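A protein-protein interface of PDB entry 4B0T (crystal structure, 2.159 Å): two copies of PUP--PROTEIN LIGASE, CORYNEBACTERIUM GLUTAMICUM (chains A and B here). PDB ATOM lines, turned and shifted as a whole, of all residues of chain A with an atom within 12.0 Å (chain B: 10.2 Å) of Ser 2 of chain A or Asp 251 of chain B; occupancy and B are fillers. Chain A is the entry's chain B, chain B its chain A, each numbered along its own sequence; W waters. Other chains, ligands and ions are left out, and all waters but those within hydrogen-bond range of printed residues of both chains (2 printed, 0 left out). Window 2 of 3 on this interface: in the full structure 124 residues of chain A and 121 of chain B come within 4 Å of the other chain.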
ATOM      1  N   SER A   2     -25.801  -7.004   0.040  1.00  0.00           N
ATOM      2  CA  SER A   2     -27.240  -6.887   0.266  1.00  0.00           C
ATOM      3  C   SER A   2     -27.926  -8.237   0.066  1.00  0.00           C
ATOM      4  O   SER A   2     -27.963  -9.052   0.989  1.00  0.00           O
ATOM      5  CB  SER A   2     -27.856  -5.823  -0.649  1.00  0.00           C
ATOM      6  OG  SER A   2     -29.136  -5.416  -0.186  1.00  0.00           O
ATOM      7  N   THR A   3     -28.444  -8.491  -1.137  1.00  0.00           N
ATOM      8  CA  THR A   3     -29.093  -9.774  -1.399  1.00  0.00           C
ATOM      9  C   THR A   3     -28.151 -10.698  -2.168  1.00  0.00           C
ATOM     10  O   THR A   3     -28.041 -10.632  -3.399  1.00  0.00           O
ATOM     11  CB  THR A   3     -30.386  -9.568  -2.211  1.00  0.00           C
ATOM     12  OG1 THR A   3     -30.093  -8.831  -3.408  1.00  0.00           O
ATOM     13  CG2 THR A   3     -31.397  -8.776  -1.389  1.00  0.00           C
ATOM     14  N   VAL A   4     -27.551 -11.631  -1.436  1.00  0.00           N
ATOM     15  CA  VAL A   4     -26.460 -12.430  -1.975  1.00  0.00           C
ATOM     16  C   VAL A   4     -26.993 -13.547  -2.846  1.00  0.00           C
ATOM     17  O   VAL A   4     -26.297 -14.027  -3.739  1.00  0.00           O
ATOM     18  CB  VAL A   4     -25.550 -13.013  -0.865  1.00  0.00           C
ATOM     19  CG1 VAL A   4     -24.665 -11.927  -0.277  1.00  0.00           C
ATOM     20  CG2 VAL A   4     -26.379 -13.684   0.220  1.00  0.00           C
ATOM     21  N   GLU A   5     -28.239 -13.939  -2.595  1.00  0.00           N
ATOM     22  CA  GLU A   5     -28.855 -15.044  -3.320  1.00  0.00           C
ATOM     23  C   GLU A   5     -29.304 -14.640  -4.713  1.00  0.00           C
ATOM     24  O   GLU A   5     -29.749 -15.479  -5.497  1.00  0.00           O
ATOM     25  CB  GLU A   5     -30.032 -15.630  -2.537  1.00  0.00           C
ATOM     26  CG  GLU A   5     -29.645 -16.315  -1.231  1.00  0.00           C
ATOM     27  CD  GLU A   5     -29.605 -15.359  -0.043  1.00  0.00           C
ATOM     28  OE1 GLU A   5     -29.269 -14.169  -0.231  1.00  0.00           O
ATOM     29  OE2 GLU A   5     -29.923 -15.801   1.083  1.00  0.00           O
ATOM     30  N   SER A   6     -29.207 -13.352  -5.016  1.00  0.00           N
ATOM     31  CA  SER A   6     -29.599 -12.865  -6.338  1.00  0.00           C
ATOM     32  C   SER A   6     -28.500 -13.031  -7.386  1.00  0.00           C
ATOM     33  O   SER A   6     -28.780 -13.016  -8.579  1.00  0.00           O
ATOM     34  CB  SER A   6     -30.060 -11.412  -6.271  1.00  0.00           C
ATOM     35  OG  SER A   6     -31.324 -11.335  -5.640  1.00  0.00           O
ATOM     36  N   ALA A   7     -27.258 -13.191  -6.935  1.00  0.00           N
ATOM     37  CA  ALA A   7     -26.139 -13.414  -7.850  1.00  0.00           C
ATOM     38  C   ALA A   7     -26.340 -14.713  -8.622  1.00  0.00           C
ATOM     39  O   ALA A   7     -26.595 -15.770  -8.024  1.00  0.00           O
ATOM     40  CB  ALA A   7     -24.822 -13.463  -7.082  1.00  0.00           C
ATOM     41  N   LEU A   8     -26.195 -14.671  -9.944  1.00  0.00           N
ATOM     42  CA  LEU A   8     -26.308 -15.926 -10.651  1.00  0.00           C
ATOM     43  C   LEU A   8     -24.894 -16.501 -10.710  1.00  0.00           C
ATOM     44  O   LEU A   8     -24.131 -16.210 -11.636  1.00  0.00           O
ATOM     45  CB  LEU A   8     -26.830 -15.674 -12.069  1.00  0.00           C
ATOM     46  CG  LEU A   8     -28.137 -14.875 -12.191  1.00  0.00           C
ATOM     47  CD1 LEU A   8     -28.510 -14.679 -13.658  1.00  0.00           C
ATOM     48  CD2 LEU A   8     -29.266 -15.562 -11.438  1.00  0.00           C
ATOM     49  N   THR A   9     -24.604 -17.417  -9.788  1.00  0.00           N
ATOM     50  CA  THR A   9     -23.279 -18.021  -9.689  1.00  0.00           C
ATOM     51  C   THR A   9     -23.229 -19.195 -10.658  1.00  0.00           C
ATOM     52  O   THR A   9     -22.170 -19.753 -10.947  1.00  0.00           O
ATOM     53  CB  THR A   9     -22.987 -18.509  -8.275  1.00  0.00           C
ATOM     54  OG1 THR A   9     -24.106 -19.277  -7.804  1.00  0.00           O
ATOM     55  CG2 THR A   9     -22.732 -17.320  -7.346  1.00  0.00           C
ATOM     56  N   ARG A  11     -24.524 -19.100 -14.476  1.00  0.00           N
ATOM     57  CA  ARG A  11     -25.183 -18.392 -15.584  1.00  0.00           C
ATOM     58  C   ARG A  11     -24.776 -18.953 -16.943  1.00  0.00           C
ATOM     59  O   ARG A  11     -23.781 -19.657 -17.055  1.00  0.00           O
ATOM     60  CB  ARG A  11     -24.958 -16.864 -15.520  1.00  0.00           C
ATOM     61  CG  ARG A  11     -23.668 -16.369 -16.134  1.00  0.00           C
ATOM     62  CD  ARG A  11     -23.560 -14.848 -16.121  1.00  0.00           C
ATOM     63  NE  ARG A  11     -23.229 -14.365 -14.779  1.00  0.00           N
ATOM     64  CZ  ARG A  11     -23.988 -13.536 -14.067  1.00  0.00           C
ATOM     65  NH1 ARG A  11     -25.117 -13.045 -14.574  1.00  0.00           N
ATOM     66  NH2 ARG A  11     -23.603 -13.172 -12.856  1.00  0.00           N
ATOM     67  N   SER B 138     -33.825  -8.794 -13.504  1.00  0.00           N
ATOM     68  CA  SER B 138     -33.528  -8.214 -12.200  1.00  0.00           C
ATOM     69  C   SER B 138     -32.582  -7.008 -12.281  1.00  0.00           C
ATOM     70  O   SER B 138     -32.900  -5.926 -11.777  1.00  0.00           O
ATOM     71  CB  SER B 138     -32.929  -9.293 -11.289  1.00  0.00           C
ATOM     72  OG  SER B 138     -31.967  -8.756 -10.394  1.00  0.00           O
ATOM     73  N   MET B 139     -31.427  -7.195 -12.921  1.00  0.00           N
ATOM     74  CA  MET B 139     -30.409  -6.145 -13.004  1.00  0.00           C
ATOM     75  C   MET B 139     -30.850  -4.916 -13.807  1.00  0.00           C
ATOM     76  O   MET B 139     -31.323  -5.043 -14.938  1.00  0.00           O
ATOM     77  CB  MET B 139     -29.111  -6.696 -13.588  1.00  0.00           C
ATOM     78  CG  MET B 139     -28.032  -5.642 -13.704  1.00  0.00           C
ATOM     79  SD  MET B 139     -26.580  -6.261 -14.540  1.00  0.00           S
ATOM     80  CE  MET B 139     -26.154  -7.648 -13.492  1.00  0.00           C
ATOM     81  N   PRO B 140     -30.667  -3.716 -13.228  1.00  0.00           N
ATOM     82  CA  PRO B 140     -31.142  -2.452 -13.812  1.00  0.00           C
ATOM     83  C   PRO B 140     -30.303  -1.977 -15.005  1.00  0.00           C
ATOM     84  O   PRO B 140     -29.095  -2.206 -15.039  1.00  0.00           O
ATOM     85  CB  PRO B 140     -31.022  -1.456 -12.648  1.00  0.00           C
ATOM     86  CG  PRO B 140     -30.451  -2.236 -11.475  1.00  0.00           C
ATOM     87  CD  PRO B 140     -29.865  -3.491 -12.015  1.00  0.00           C
ATOM     88  N   ALA B 143     -27.182   0.360 -13.989  1.00  0.00           N
ATOM     89  CA  ALA B 143     -25.972  -0.166 -13.357  1.00  0.00           C
ATOM     90  C   ALA B 143     -24.832  -0.404 -14.334  1.00  0.00           C
ATOM     91  O   ALA B 143     -23.660  -0.281 -13.973  1.00  0.00           O
ATOM     92  CB  ALA B 143     -26.280  -1.441 -12.594  1.00  0.00           C
ATOM     93  N   ARG B 147     -21.379   0.757 -13.200  1.00  0.00           N
ATOM     94  CA  ARG B 147     -20.550  -0.245 -12.539  1.00  0.00           C
ATOM     95  C   ARG B 147     -19.757  -1.132 -13.511  1.00  0.00           C
ATOM     96  O   ARG B 147     -18.530  -1.202 -13.440  1.00  0.00           O
ATOM     97  CB  ARG B 147     -21.364  -1.021 -11.495  1.00  0.00           C
ATOM     98  CG  ARG B 147     -21.626  -0.167 -10.259  1.00  0.00           C
ATOM     99  CD  ARG B 147     -22.810  -0.636  -9.442  1.00  0.00           C
ATOM    100  NE  ARG B 147     -22.916   0.132  -8.207  1.00  0.00           N
ATOM    101  CZ  ARG B 147     -23.680   1.212  -8.053  1.00  0.00           C
ATOM    102  NH1 ARG B 147     -24.417   1.665  -9.059  1.00  0.00           N
ATOM    103  NH2 ARG B 147     -23.710   1.839  -6.885  1.00  0.00           N
ATOM    104  N   LEU B 243     -17.554 -12.135 -11.743  1.00  0.00           N
ATOM    105  CA  LEU B 243     -17.586 -11.598 -10.389  1.00  0.00           C
ATOM    106  C   LEU B 243     -18.223 -10.206 -10.352  1.00  0.00           C
ATOM    107  O   LEU B 243     -19.031  -9.913  -9.483  1.00  0.00           O
ATOM    108  CB  LEU B 243     -16.170 -11.552  -9.804  1.00  0.00           C
ATOM    109  CG  LEU B 243     -15.541 -12.925  -9.532  1.00  0.00           C
ATOM    110  CD1 LEU B 243     -14.047 -12.790  -9.353  1.00  0.00           C
ATOM    111  CD2 LEU B 243     -16.150 -13.585  -8.303  1.00  0.00           C
ATOM    112  N   VAL B 244     -17.865  -9.353 -11.303  1.00  0.00           N
ATOM    113  CA  VAL B 244     -18.442  -8.013 -11.357  1.00  0.00           C
ATOM    114  C   VAL B 244     -19.952  -8.089 -11.560  1.00  0.00           C
ATOM    115  O   VAL B 244     -20.709  -7.384 -10.884  1.00  0.00           O
ATOM    116  CB  VAL B 244     -17.805  -7.148 -12.451  1.00  0.00           C
ATOM    117  CG1 VAL B 244     -18.537  -5.811 -12.560  1.00  0.00           C
ATOM    118  CG2 VAL B 244     -16.310  -6.932 -12.151  1.00  0.00           C
ATOM    119  N   LEU B 245     -20.398  -8.966 -12.458  1.00  0.00           N
ATOM    120  CA  LEU B 245     -21.838  -9.137 -12.672  1.00  0.00           C
ATOM    121  C   LEU B 245     -22.556  -9.622 -11.416  1.00  0.00           C
ATOM    122  O   LEU B 245     -23.665  -9.174 -11.115  1.00  0.00           O
ATOM    123  CB  LEU B 245     -22.130 -10.073 -13.857  1.00  0.00           C
ATOM    124  CG  LEU B 245     -21.602  -9.663 -15.241  1.00  0.00           C
ATOM    125  CD1 LEU B 245     -21.877 -10.782 -16.237  1.00  0.00           C
ATOM    126  CD2 LEU B 245     -22.228  -8.348 -15.726  1.00  0.00           C
ATOM    127  N   GLU B 246     -21.933 -10.546 -10.691  1.00  0.00           N
ATOM    128  CA  GLU B 246     -22.541 -11.084  -9.473  1.00  0.00           C
ATOM    129  C   GLU B 246     -22.685  -9.997  -8.405  1.00  0.00           C
ATOM    130  O   GLU B 246     -23.727  -9.878  -7.782  1.00  0.00           O
ATOM    131  CB  GLU B 246     -21.732 -12.267  -8.924  1.00  0.00           C
ATOM    132  CG  GLU B 246     -21.591 -13.435  -9.903  1.00  0.00           C
ATOM    133  CD  GLU B 246     -20.684 -14.554  -9.369  1.00  0.00           C
ATOM    134  OE1 GLU B 246     -20.126 -14.403  -8.253  1.00  0.00           O
ATOM    135  OE2 GLU B 246     -20.527 -15.578 -10.075  1.00  0.00           O
ATOM    136  N   MET B 247     -21.627  -9.221  -8.196  1.00  0.00           N
ATOM    137  CA  MET B 247     -21.673  -8.120  -7.245  1.00  0.00           C
ATOM    138  C   MET B 247     -22.798  -7.134  -7.579  1.00  0.00           C
ATOM    139  O   MET B 247     -23.548  -6.724  -6.699  1.00  0.00           O
ATOM    140  CB  MET B 247     -20.330  -7.394  -7.196  1.00  0.00           C
ATOM    141  CG  MET B 247     -19.236  -8.190  -6.517  1.00  0.00           C
ATOM    142  SD  MET B 247     -17.766  -7.211  -6.140  1.00  0.00           S
ATOM    143  CE  MET B 247     -17.091  -6.894  -7.778  1.00  0.00           C
ATOM    144  N   ILE B 248     -22.910  -6.757  -8.851  1.00  0.00           N
ATOM    145  CA  ILE B 248     -24.016  -5.917  -9.282  1.00  0.00           C
ATOM    146  C   ILE B 248     -25.365  -6.576  -8.966  1.00  0.00           C
ATOM    147  O   ILE B 248     -26.222  -5.971  -8.323  1.00  0.00           O
ATOM    148  CB  ILE B 248     -23.925  -5.566 -10.782  1.00  0.00           C
ATOM    149  CG1 ILE B 248     -22.656  -4.764 -11.059  1.00  0.00           C
ATOM    150  CG2 ILE B 248     -25.121  -4.747 -11.214  1.00  0.00           C
ATOM    151  CD1 ILE B 248     -22.434  -4.479 -12.534  1.00  0.00           C
ATOM    152  N   GLU B 249     -25.546  -7.816  -9.409  1.00  0.00           N
ATOM    153  CA  GLU B 249     -26.783  -8.557  -9.156  1.00  0.00           C
ATOM    154  C   GLU B 249     -27.103  -8.675  -7.657  1.00  0.00           C
ATOM    155  O   GLU B 249     -28.270  -8.705  -7.268  1.00  0.00           O
ATOM    156  CB  GLU B 249     -26.724  -9.958  -9.800  1.00  0.00           C
ATOM    157  CG  GLU B 249     -26.877  -9.950 -11.321  1.00  0.00           C
ATOM    158  CD  GLU B 249     -26.483 -11.278 -12.012  1.00  0.00           C
ATOM    159  OE1 GLU B 249     -25.803 -12.144 -11.408  1.00  0.00           O
ATOM    160  OE2 GLU B 249     -26.863 -11.444 -13.185  1.00  0.00           O
ATOM    161  N   ALA B 250     -26.066  -8.757  -6.827  1.00  0.00           N
ATOM    162  CA  ALA B 250     -26.246  -8.963  -5.391  1.00  0.00           C
ATOM    163  C   ALA B 250     -26.354  -7.632  -4.638  1.00  0.00           C
ATOM    164  O   ALA B 250     -26.564  -7.610  -3.424  1.00  0.00           O
ATOM    165  CB  ALA B 250     -25.094  -9.810  -4.823  1.00  0.00           C
ATOM    166  N   ASP B 251     -26.212  -6.529  -5.367  1.00  0.00           N
ATOM    167  CA  ASP B 251     -26.226  -5.218  -4.757  1.00  0.00           C
ATOM    168  C   ASP B 251     -25.206  -5.212  -3.623  1.00  0.00           C
ATOM    169  O   ASP B 251     -25.520  -4.831  -2.493  1.00  0.00           O
ATOM    170  CB  ASP B 251     -27.627  -4.897  -4.225  1.00  0.00           C
ATOM    171  CG  ASP B 251     -27.771  -3.446  -3.792  1.00  0.00           C
ATOM    172  OD1 ASP B 251     -27.032  -2.582  -4.322  1.00  0.00           O
ATOM    173  OD2 ASP B 251     -28.630  -3.165  -2.924  1.00  0.00           O
ATOM    174  N   PHE B 252     -23.984  -5.637  -3.934  1.00  0.00           N
ATOM    175  CA  PHE B 252     -22.981  -5.887  -2.908  1.00  0.00           C
ATOM    176  C   PHE B 252     -22.227  -4.629  -2.475  1.00  0.00           C
ATOM    177  O   PHE B 252     -21.414  -4.675  -1.551  1.00  0.00           O
ATOM    178  CB  PHE B 252     -22.013  -6.976  -3.384  1.00  0.00           C
ATOM    179  CG  PHE B 252     -20.945  -7.328  -2.389  1.00  0.00           C
ATOM    180  CD1 PHE B 252     -21.251  -8.050  -1.253  1.00  0.00           C
ATOM    181  CD2 PHE B 252     -19.627  -6.950  -2.606  1.00  0.00           C
ATOM    182  CE1 PHE B 252     -20.267  -8.381  -0.341  1.00  0.00           C
ATOM    183  CE2 PHE B 252     -18.632  -7.280  -1.697  1.00  0.00           C
ATOM    184  CZ  PHE B 252     -18.953  -7.999  -0.564  1.00  0.00           C
ATOM    185  N   GLY B 253     -22.514  -3.499  -3.115  1.00  0.00           N
ATOM    186  CA  GLY B 253     -21.896  -2.243  -2.713  1.00  0.00           C
ATOM    187  C   GLY B 253     -20.704  -1.766  -3.532  1.00  0.00           C
ATOM    188  O   GLY B 253     -19.935  -0.910  -3.086  1.00  0.00           O
ATOM    189  N   LEU B 254     -20.525  -2.334  -4.720  1.00  0.00           N
ATOM    190  CA  LEU B 254     -19.560  -1.802  -5.677  1.00  0.00           C
ATOM    191  C   LEU B 254     -19.863  -0.327  -5.927  1.00  0.00           C
ATOM    192  O   LEU B 254     -20.994   0.038  -6.272  1.00  0.00           O
ATOM    193  CB  LEU B 254     -19.651  -2.586  -6.977  1.00  0.00           C
ATOM    194  CG  LEU B 254     -18.452  -2.611  -7.915  1.00  0.00           C
ATOM    195  CD1 LEU B 254     -17.203  -3.105  -7.192  1.00  0.00           C
ATOM    196  CD2 LEU B 254     -18.787  -3.501  -9.099  1.00  0.00           C
ATOM    197  N   PRO B 255     -18.860   0.536  -5.733  1.00  0.00           N
ATOM    198  CA  PRO B 255     -19.092   1.979  -5.871  1.00  0.00           C
ATOM    199  C   PRO B 255     -19.398   2.323  -7.311  1.00  0.00           C
ATOM    200  O   PRO B 255     -18.982   1.579  -8.210  1.00  0.00           O
ATOM    201  CB  PRO B 255     -17.741   2.594  -5.480  1.00  0.00           C
ATOM    202  CG  PRO B 255     -17.043   1.531  -4.688  1.00  0.00           C
ATOM    203  CD  PRO B 255     -17.493   0.230  -5.288  1.00  0.00           C
ATOM    204  N   SER B 256     -20.078   3.442  -7.537  1.00  0.00           N
ATOM    205  CA  SER B 256     -20.291   3.891  -8.899  1.00  0.00           C
ATOM    206  C   SER B 256     -19.055   4.662  -9.331  1.00  0.00           C
ATOM    207  O   SER B 256     -18.681   5.672  -8.741  1.00  0.00           O
ATOM    208  CB  SER B 256     -21.527   4.782  -9.003  1.00  0.00           C
ATOM    209  OG  SER B 256     -21.589   5.381 -10.286  1.00  0.00           O
ATOM    210  N   HIS B 299     -13.195  -5.163  -3.834  1.00  0.00           N
ATOM    211  CA  HIS B 299     -14.585  -5.524  -3.573  1.00  0.00           C
ATOM    212  C   HIS B 299     -14.886  -6.962  -3.997  1.00  0.00           C
ATOM    213  O   HIS B 299     -15.627  -7.686  -3.316  1.00  0.00           O
ATOM    214  CB  HIS B 299     -15.544  -4.543  -4.242  1.00  0.00           C
ATOM    215  CG  HIS B 299     -15.670  -3.242  -3.513  1.00  0.00           C
ATOM    216  ND1 HIS B 299     -15.069  -2.079  -3.949  1.00  0.00           N
ATOM    217  CD2 HIS B 299     -16.312  -2.925  -2.364  1.00  0.00           C
ATOM    218  CE1 HIS B 299     -15.348  -1.099  -3.109  1.00  0.00           C
ATOM    219  NE2 HIS B 299     -16.100  -1.585  -2.138  1.00  0.00           N
ATOM    220  N   LYS B 302     -13.786  -9.298  -1.359  1.00  0.00           N
ATOM    221  CA  LYS B 302     -14.707  -9.406  -0.239  1.00  0.00           C
ATOM    222  C   LYS B 302     -15.962 -10.174  -0.637  1.00  0.00           C
ATOM    223  O   LYS B 302     -16.531 -10.907   0.171  1.00  0.00           O
ATOM    224  CB  LYS B 302     -15.038  -8.028   0.346  1.00  0.00           C
ATOM    225  CG  LYS B 302     -13.845  -7.379   1.031  1.00  0.00           C
ATOM    226  CD  LYS B 302     -14.238  -6.120   1.787  1.00  0.00           C
ATOM    227  CE  LYS B 302     -13.096  -5.627   2.675  1.00  0.00           C
ATOM    228  NZ  LYS B 302     -12.784  -6.585   3.781  1.00  0.00           N
ATOM    229  N   TRP B 303     -16.387 -10.014  -1.886  1.00  0.00           N
ATOM    230  CA  TRP B 303     -17.530 -10.778  -2.387  1.00  0.00           C
ATOM    231  C   TRP B 303     -17.293 -12.267  -2.204  1.00  0.00           C
ATOM    232  O   TRP B 303     -18.170 -12.987  -1.718  1.00  0.00           O
ATOM    233  CB  TRP B 303     -17.816 -10.447  -3.856  1.00  0.00           C
ATOM    234  CG  TRP B 303     -18.769 -11.396  -4.543  1.00  0.00           C
ATOM    235  CD1 TRP B 303     -18.515 -12.135  -5.663  1.00  0.00           C
ATOM    236  CD2 TRP B 303     -20.116 -11.708  -4.157  1.00  0.00           C
ATOM    237  NE1 TRP B 303     -19.618 -12.881  -6.004  1.00  0.00           N
ATOM    238  CE2 TRP B 303     -20.614 -12.639  -5.096  1.00  0.00           C
ATOM    239  CE3 TRP B 303     -20.949 -11.289  -3.112  1.00  0.00           C
ATOM    240  CZ2 TRP B 303     -21.902 -13.161  -5.021  1.00  0.00           C
ATOM    241  CZ3 TRP B 303     -22.229 -11.805  -3.039  1.00  0.00           C
ATOM    242  CH2 TRP B 303     -22.694 -12.737  -3.987  1.00  0.00           C
ATOM    243  N   GLN B 306     -18.263 -13.865   1.014  1.00  0.00           N
ATOM    244  CA  GLN B 306     -19.702 -14.098   1.141  1.00  0.00           C
ATOM    245  C   GLN B 306     -20.373 -14.847  -0.021  1.00  0.00           C
ATOM    246  O   GLN B 306     -21.574 -15.110   0.025  1.00  0.00           O
ATOM    247  CB  GLN B 306     -20.424 -12.773   1.361  1.00  0.00           C
ATOM    248  CG  GLN B 306     -19.977 -12.038   2.596  1.00  0.00           C
ATOM    249  CD  GLN B 306     -20.763 -10.769   2.813  1.00  0.00           C
ATOM    250  OE1 GLN B 306     -20.184  -9.703   3.005  1.00  0.00           O
ATOM    251  NE2 GLN B 306     -22.093 -10.874   2.782  1.00  0.00           N
ATOM    252  N   PRO B 308     -22.126 -17.314  -2.104  1.00  0.00           N
ATOM    253  CA  PRO B 308     -22.719 -18.632  -1.869  1.00  0.00           C
ATOM    254  C   PRO B 308     -22.269 -19.612  -2.938  1.00  0.00           C
ATOM    255  O   PRO B 308     -22.284 -19.276  -4.124  1.00  0.00           O
ATOM    256  CB  PRO B 308     -24.230 -18.374  -1.988  1.00  0.00           C
ATOM    257  CG  PRO B 308     -24.383 -16.887  -1.859  1.00  0.00           C
ATOM    258  CD  PRO B 308     -23.138 -16.297  -2.435  1.00  0.00           C
HETATM  259  O   HOH W   1     -24.596 -19.182  -5.128  1.00  0.00           O
HETATM  260  O   HOH W   2     -21.525 -15.748 -12.612  1.00  0.00           O
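OE2 of Glu 249 of chain B lies within salt-bridge range of NH1 of Arg 11 of chain A (2.7 Å).
The side-chain carboxylate (OE1) of Glu 249 of chain B sits at hydrogen-bond distance from the backbone NH (N) of Leu 8 of chain A, at 2.9 Å.
The backbone carbonyl oxygen of Asp 251 of chain B sits close to the backbone NH of Ser 2 of chain A (3.3 Å).
N of Thr 3 of chain A is in hydrogen-bond range of O of Ala 250 of chain B.
The side-chain carboxylate of Glu 246 of chain B is in hydrogen-bond range of the indole nitrogen of Trp 303 of chain B (2.8 Å).
O of Leu 8 of chain A sits at hydrogen-bond distance from NH2 of Arg 11 of chain A.
Ala 250 of chain B touches Ser 2 of chain A.
Val 4 of chain A touches Trp 303 of chain B (CG1 to CZ3, 3.7 Å).
Pro 308 of chain B touches Val 4 of chain A (CG to O, 3.9 Å).
Glu 249 of chain B touches Ser 6 of chain A.
CB of Ala 7 of chain A touches CB of Glu 246 of chain B, at 3.8 Å.
Ala 7 of chain A touches Glu 249 of chain B (CA to OE1, 3.8 Å).
Trp 303 of chain B touches Ala 7 of chain A.
Leu 8 of chain A touches Glu 246 of chain B (O to OE2, 3.98 Å).
Thr 9 of chain A touches Glu 246 of chain B.
Pro 308 of chain B touches Thr 9 of chain A.
Of the printed residues of chain B, Ser 2 of chain A touches Ala 250 (3.5 Å) and Asp 251 (3.1 Å).
Asp 251 of chain B touches just one residue of chain A: Ser 2 (3.1 Å).
Thr 3 of chain A touches one residue of chain B.
Of chain A, only Ser 2 (3.5 Å) and Thr 3 (3.1 Å) come within 4 Å of Ala 250 of chain B.
No residue of chain A comes within 4 Å of Phe 252 of chain B.
No residue of chain A comes within 4 Å of Gly 253 of chain B.
Printed residues of chain A within 4 Å of Trp 303 of chain B: Val 4 and Ala 7.
Of the printed residues of chain A, Glu 246 of chain B touches Ala 7 (3.8 Å), Leu 8 (3.98 Å), Thr 9 (3.7 Å) and Arg 11 (3.6 Å).
Of the printed residues of chain B, Ala 7 of chain A touches Glu 246 (3.8 Å), Glu 249 (3.8 Å) and Trp 303 (3.6 Å).
Printed residues of chain A within 4 Å of Glu 249 of chain B: Ser 6 (3.4 Å), Ala 7 (3.8 Å), Leu 8 (2.9 Å) and Arg 11 (2.7 Å).
Pro 255 of chain B touches none of the printed residues of chain A.
The nearest residue of chain A that does not touch Asp 251 of chain B is Thr 3 of chain A (4.7 Å).
Of the 24 printed residues of chain B, 7 touch a printed residue of chain A.
Printed residues of chain B that touch a printed residue of chain A: Leu 245, Glu 246, Glu 249, Ala 250, Asp 251, Trp 303 and Pro 308.
Hydrophobic or aromatic side chains of chain B within 4 Å of the printed part of chain A: Leu 245, Ala 250, Trp 303 and Pro 308.
Of the 9 printed residues of chain A, 8 touch a printed residue of chain B.
Hydrophobic or aromatic side chains of chain A that line the printed part of chain B: Val 4, Ala 7 and Leu 8.
Along chain A the printed residues that touch a printed residue of chain B span positions 2 to 11.
Among the printed residues, Asp or Glu carboxylates within 4 Å of a Lys or Arg side-chain nitrogen of the other chain: Arg 11 of chain A with Glu 249 of chain B (2.7 Å).
No position is printed for both chains.
Water W1 lies within hydrogen-bond range of O of Pro 308 of chain B (2.5 Å) and OG1 of Thr 9 of chain A (2.7 Å).
Water W2 lies within hydrogen-bond range of the side-chain carboxylate (OE2) of Glu 246 of chain B, the backbone carbonyl oxygen (O) of Leu 8 of chain A and the guanidinium group (NE) of Arg 11 of chain A.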
